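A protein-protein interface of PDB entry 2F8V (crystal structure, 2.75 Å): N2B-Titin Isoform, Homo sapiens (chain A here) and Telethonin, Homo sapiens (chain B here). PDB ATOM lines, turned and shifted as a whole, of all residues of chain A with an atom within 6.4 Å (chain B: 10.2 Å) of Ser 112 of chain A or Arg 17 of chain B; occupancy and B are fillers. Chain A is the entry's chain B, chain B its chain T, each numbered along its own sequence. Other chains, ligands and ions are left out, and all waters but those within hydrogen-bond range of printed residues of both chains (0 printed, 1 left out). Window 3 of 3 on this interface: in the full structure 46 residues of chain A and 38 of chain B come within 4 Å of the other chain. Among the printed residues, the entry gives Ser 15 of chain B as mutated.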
ATOM      1  N   LEU A 110      -1.533  25.602  17.627  1.00  0.00           N
ATOM      2  CA  LEU A 110      -0.729  26.376  16.701  1.00  0.00           C
ATOM      3  C   LEU A 110       0.410  25.455  16.378  1.00  0.00           C
ATOM      4  O   LEU A 110       0.713  24.564  17.154  1.00  0.00           O
ATOM      5  CB  LEU A 110      -0.208  27.593  17.415  1.00  0.00           C
ATOM      6  CG  LEU A 110      -0.228  28.917  16.671  1.00  0.00           C
ATOM      7  CD1 LEU A 110      -1.531  29.072  16.003  1.00  0.00           C
ATOM      8  CD2 LEU A 110       0.023  30.093  17.653  1.00  0.00           C
ATOM      9  N   GLN A 111       1.060  25.649  15.245  1.00  0.00           N
ATOM     10  CA  GLN A 111       2.037  24.671  14.800  1.00  0.00           C
ATOM     11  C   GLN A 111       3.193  25.370  14.098  1.00  0.00           C
ATOM     12  O   GLN A 111       2.983  26.075  13.113  1.00  0.00           O
ATOM     13  CB  GLN A 111       1.331  23.728  13.842  1.00  0.00           C
ATOM     14  CG  GLN A 111       1.963  22.391  13.733  1.00  0.00           C
ATOM     15  CD  GLN A 111       1.111  21.240  14.215  1.00  0.00           C
ATOM     16  OE1 GLN A 111      -0.090  21.165  13.932  1.00  0.00           O
ATOM     17  NE2 GLN A 111       1.751  20.301  14.902  1.00  0.00           N
ATOM     18  N   SER A 112       4.409  25.187  14.612  1.00  0.00           N
ATOM     19  CA  SER A 112       5.585  25.866  14.075  1.00  0.00           C
ATOM     20  C   SER A 112       5.798  25.520  12.639  1.00  0.00           C
ATOM     21  O   SER A 112       5.620  24.376  12.264  1.00  0.00           O
ATOM     22  CB  SER A 112       6.816  25.454  14.860  1.00  0.00           C
ATOM     23  OG  SER A 112       6.875  26.189  16.063  1.00  0.00           O
ATOM     24  N   MET A 113       6.195  26.491  11.830  1.00  0.00           N
ATOM     25  CA  MET A 113       6.427  26.211  10.411  1.00  0.00           C
ATOM     26  C   MET A 113       7.474  27.080   9.720  1.00  0.00           C
ATOM     27  O   MET A 113       7.617  28.252  10.032  1.00  0.00           O
ATOM     28  CB  MET A 113       5.106  26.152   9.622  1.00  0.00           C
ATOM     29  CG  MET A 113       4.317  27.417   9.524  1.00  0.00           C
ATOM     30  SD  MET A 113       2.730  27.143   8.616  1.00  0.00           S
ATOM     31  CE  MET A 113       1.672  26.409   9.861  1.00  0.00           C
ATOM     32  N   THR A 114       8.200  26.483   8.776  1.00  0.00           N
ATOM     33  CA  THR A 114       9.237  27.177   8.001  1.00  0.00           C
ATOM     34  C   THR A 114       8.789  27.429   6.582  1.00  0.00           C
ATOM     35  O   THR A 114       8.384  26.511   5.887  1.00  0.00           O
ATOM     36  CB  THR A 114      10.513  26.326   7.913  1.00  0.00           C
ATOM     37  OG1 THR A 114      10.861  25.841   9.212  1.00  0.00           O
ATOM     38  CG2 THR A 114      11.699  27.170   7.478  1.00  0.00           C
ATOM     39  N   THR A 188       1.571  28.413  21.838  1.00  0.00           N
ATOM     40  CA  THR A 188       2.576  29.211  21.143  1.00  0.00           C
ATOM     41  C   THR A 188       3.370  28.377  20.140  1.00  0.00           C
ATOM     42  O   THR A 188       3.669  27.227  20.405  1.00  0.00           O
ATOM     43  CB  THR A 188       3.455  30.059  22.130  1.00  0.00           C
ATOM     44  OG1 THR A 188       4.703  29.409  22.421  1.00  0.00           O
ATOM     45  CG2 THR A 188       2.774  30.202  23.484  1.00  0.00           C
ATOM     46  N   ALA A 189       3.661  28.939  18.974  1.00  0.00           N
ATOM     47  CA  ALA A 189       4.503  28.275  17.978  1.00  0.00           C
ATOM     48  C   ALA A 189       5.432  29.275  17.288  1.00  0.00           C
ATOM     49  O   ALA A 189       5.322  30.491  17.503  1.00  0.00           O
ATOM     50  CB  ALA A 189       3.664  27.554  16.952  1.00  0.00           C
ATOM     51  N   GLU A 190       6.327  28.764  16.449  1.00  0.00           N
ATOM     52  CA  GLU A 190       7.234  29.635  15.734  1.00  0.00           C
ATOM     53  C   GLU A 190       7.183  29.587  14.232  1.00  0.00           C
ATOM     54  O   GLU A 190       6.929  28.548  13.640  1.00  0.00           O
ATOM     55  CB  GLU A 190       8.645  29.445  16.217  1.00  0.00           C
ATOM     56  CG  GLU A 190       8.898  30.332  17.418  1.00  0.00           C
ATOM     57  CD  GLU A 190      10.168  31.095  17.257  1.00  0.00           C
ATOM     58  OE1 GLU A 190      10.710  31.066  16.145  1.00  0.00           O
ATOM     59  OE2 GLU A 190      10.624  31.713  18.225  1.00  0.00           O
ATOM     60  N   LEU A 191       7.433  30.735  13.625  1.00  0.00           N
ATOM     61  CA  LEU A 191       7.377  30.871  12.177  1.00  0.00           C
ATOM     62  C   LEU A 191       8.706  31.354  11.638  1.00  0.00           C
ATOM     63  O   LEU A 191       9.200  32.404  12.022  1.00  0.00           O
ATOM     64  CB  LEU A 191       6.311  31.890  11.804  1.00  0.00           C
ATOM     65  CG  LEU A 191       6.229  32.261  10.329  1.00  0.00           C
ATOM     66  CD1 LEU A 191       5.540  31.147   9.526  1.00  0.00           C
ATOM     67  CD2 LEU A 191       5.513  33.591  10.148  1.00  0.00           C
ATOM     68  N   GLU B  13       5.979  21.921  26.838  1.00  0.00           N
ATOM     69  CA  GLU B  13       6.848  22.579  25.860  1.00  0.00           C
ATOM     70  C   GLU B  13       7.537  21.575  24.942  1.00  0.00           C
ATOM     71  O   GLU B  13       7.794  20.434  25.327  1.00  0.00           O
ATOM     72  CB  GLU B  13       7.886  23.422  26.568  1.00  0.00           C
ATOM     73  CG  GLU B  13       8.940  22.602  27.265  1.00  0.00           C
ATOM     74  CD  GLU B  13      10.053  22.188  26.329  1.00  0.00           C
ATOM     75  OE1 GLU B  13       9.961  22.521  25.121  1.00  0.00           O
ATOM     76  OE2 GLU B  13      11.017  21.544  26.806  1.00  0.00           O
ATOM     77  N   ASN B  14       7.830  22.005  23.720  1.00  0.00           N
ATOM     78  CA  ASN B  14       8.499  21.170  22.731  1.00  0.00           C
ATOM     79  C   ASN B  14       9.640  21.933  22.064  1.00  0.00           C
ATOM     80  O   ASN B  14       9.413  22.833  21.287  1.00  0.00           O
ATOM     81  CB  ASN B  14       7.510  20.657  21.682  1.00  0.00           C
ATOM     82  CG  ASN B  14       8.197  19.897  20.547  1.00  0.00           C
ATOM     83  OD1 ASN B  14       9.311  20.232  20.157  1.00  0.00           O
ATOM     84  ND2 ASN B  14       7.532  18.875  20.018  1.00  0.00           N
ATOM     85  N   SER B  15      10.872  21.542  22.368  1.00  0.00           N
ATOM     86  CA  SER B  15      12.045  22.264  21.883  1.00  0.00           C
ATOM     87  C   SER B  15      12.495  21.838  20.499  1.00  0.00           C
ATOM     88  O   SER B  15      13.280  22.530  19.866  1.00  0.00           O
ATOM     89  CB  SER B  15      13.198  22.138  22.870  1.00  0.00           C
ATOM     90  OG  SER B  15      13.086  20.935  23.579  1.00  0.00           O
ATOM     91  N   GLU B  16      12.001  20.693  20.045  1.00  0.00           N
ATOM     92  CA  GLU B  16      12.301  20.233  18.705  1.00  0.00           C
ATOM     93  C   GLU B  16      11.580  21.107  17.696  1.00  0.00           C
ATOM     94  O   GLU B  16      12.083  21.338  16.605  1.00  0.00           O
ATOM     95  CB  GLU B  16      11.884  18.788  18.552  1.00  0.00           C
ATOM     96  CG  GLU B  16      12.022  18.229  17.148  1.00  0.00           C
ATOM     97  CD  GLU B  16      11.561  16.776  17.088  1.00  0.00           C
ATOM     98  OE1 GLU B  16      10.332  16.521  17.106  1.00  0.00           O
ATOM     99  OE2 GLU B  16      12.423  15.877  17.064  1.00  0.00           O
ATOM    100  N   ARG B  17      10.412  21.620  18.065  1.00  0.00           N
ATOM    101  CA  ARG B  17       9.607  22.438  17.156  1.00  0.00           C
ATOM    102  C   ARG B  17       9.418  23.846  17.678  1.00  0.00           C
ATOM    103  O   ARG B  17       8.867  24.699  16.988  1.00  0.00           O
ATOM    104  CB  ARG B  17       8.228  21.812  16.943  1.00  0.00           C
ATOM    105  CG  ARG B  17       8.228  20.383  16.393  1.00  0.00           C
ATOM    106  CD  ARG B  17       8.359  20.291  14.883  1.00  0.00           C
ATOM    107  NE  ARG B  17       7.379  21.082  14.134  1.00  0.00           N
ATOM    108  CZ  ARG B  17       6.068  21.163  14.398  1.00  0.00           C
ATOM    109  NH1 ARG B  17       5.505  20.509  15.419  1.00  0.00           N
ATOM    110  NH2 ARG B  17       5.302  21.916  13.620  1.00  0.00           N
ATOM    111  N   ARG B  18       9.891  24.096  18.890  1.00  0.00           N
ATOM    112  CA  ARG B  18       9.703  25.395  19.534  1.00  0.00           C
ATOM    113  C   ARG B  18       8.225  25.714  19.642  1.00  0.00           C
ATOM    114  O   ARG B  18       7.764  26.707  19.091  1.00  0.00           O
ATOM    115  CB  ARG B  18      10.409  26.506  18.765  1.00  0.00           C
ATOM    116  CG  ARG B  18      11.879  26.267  18.538  1.00  0.00           C
ATOM    117  CD  ARG B  18      12.759  26.703  19.697  1.00  0.00           C
ATOM    118  NE  ARG B  18      13.378  25.591  20.413  1.00  0.00           N
ATOM    119  CZ  ARG B  18      14.453  25.740  21.159  1.00  0.00           C
ATOM    120  NH1 ARG B  18      14.993  26.940  21.258  1.00  0.00           N
ATOM    121  NH2 ARG B  18      14.990  24.723  21.795  1.00  0.00           N
ATOM    122  N   GLU B  19       7.488  24.855  20.333  1.00  0.00           N
ATOM    123  CA  GLU B  19       6.051  25.033  20.545  1.00  0.00           C
ATOM    124  C   GLU B  19       5.814  24.881  22.027  1.00  0.00           C
ATOM    125  O   GLU B  19       6.492  24.102  22.672  1.00  0.00           O
ATOM    126  CB  GLU B  19       5.243  23.975  19.794  1.00  0.00           C
ATOM    127  CG  GLU B  19       5.341  24.102  18.291  1.00  0.00           C
ATOM    128  CD  GLU B  19       4.936  22.849  17.546  1.00  0.00           C
ATOM    129  OE1 GLU B  19       4.805  21.806  18.178  1.00  0.00           O
ATOM    130  OE2 GLU B  19       4.751  22.901  16.314  1.00  0.00           O
ATOM    131  N   ALA B  20       4.872  25.638  22.575  1.00  0.00           N
ATOM    132  CA  ALA B  20       4.527  25.496  23.978  1.00  0.00           C
ATOM    133  C   ALA B  20       3.018  25.546  24.127  1.00  0.00           C
ATOM    134  O   ALA B  20       2.314  25.872  23.166  1.00  0.00           O
ATOM    135  CB  ALA B  20       5.201  26.576  24.803  1.00  0.00           C
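OG of Ser 112 of chain A is in hydrogen-bond range of O of Arg 17 of chain B (2.7 Å).
OG of Ser 112 of chain A sits at hydrogen-bond distance from O of Arg 18 of chain B (3.2 Å).
The backbone NH (N) of Ser 112 of chain A is in hydrogen-bond range of the side-chain carboxylate (OE2) of Glu 19 of chain B, 2.9 Å away.
O of Thr 188 of chain A is in hydrogen-bond range of N of Ala 20 of chain B (2.9 Å).
The side-chain hydroxyl (OG) of Ser 112 of chain A is in hydrogen-bond range of the backbone NH (N) of Glu 190 of chain A (2.7 Å).
O of Glu 190 of chain A lies within hydrogen-bond range of N of Met 113 of chain A, 2.8 Å away.
The backbone NH (N) of Arg 17 of chain B sits at hydrogen-bond distance from the side-chain amide oxygen (OD1) of Asn 14 of chain B, at 2.7 Å.
O of Glu 19 of chain B is in hydrogen-bond range of N of Asn 14 of chain B (2.7 Å).
The backbone carbonyl oxygen (O) of Ser 15 of chain B lies within hydrogen-bond range of the guanidinium group (NE) of Arg 18 of chain B (3.1 Å).
The side-chain carboxylate (OE2) of Glu 19 of chain B is in salt-bridge range of the guanidinium group (NH1) of Arg 17 of chain B, 2.7 Å away.
Among the printed residues, pairs that only touch across the chains: Thr 188 of chain A with Glu 19 of chain B (3.2 Å), Gln 111 of chain A with Arg 17 of chain B (3.4 Å), Gln 111 of chain A with Glu 19 of chain B (3.6 Å), Glu 190 of chain A with Arg 18 of chain B (3.6 Å) and Ala 189 of chain A with Arg 18 of chain B (3.8 Å).
Ser 112 of chain A touches just these residues of chain B: Arg 17, Arg 18 and Glu 19.
Printed residues of chain A within 4 Å of Arg 17 of chain B: Gln 111 and Ser 112.
Of chain B, only Arg 17 (3.4 Å) and Glu 19 (3.6 Å) come within 4 Å of Gln 111 of chain A.
Printed residues of chain A within 4 Å of Arg 18 of chain B: Ser 112, Ala 189 and Glu 190.
Printed residues of chain A within 4 Å of Glu 19 of chain B: Gln 111, Ser 112 and Thr 188.
Ser 15 of chain B touches none of the printed residues of chain A.
The nearest residue of chain B that does not touch Ser 112 of chain A is Asn 14 of chain B (6.7 Å).
The nearest printed residue of chain B that does not touch Thr 188 of chain A is Arg 18 of chain B (4.3 Å).
Along chain A the printed residues that touch a printed residue of chain B span positions 111 to 190.
Printed residues of chain B that touch a printed residue of chain A: Arg 17, Arg 18, Glu 19 and Ala 20.
Among the printed residues, no Asp or Glu carboxylate lies within 4 Å of a Lys or Arg side-chain nitrogen of the other chain.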
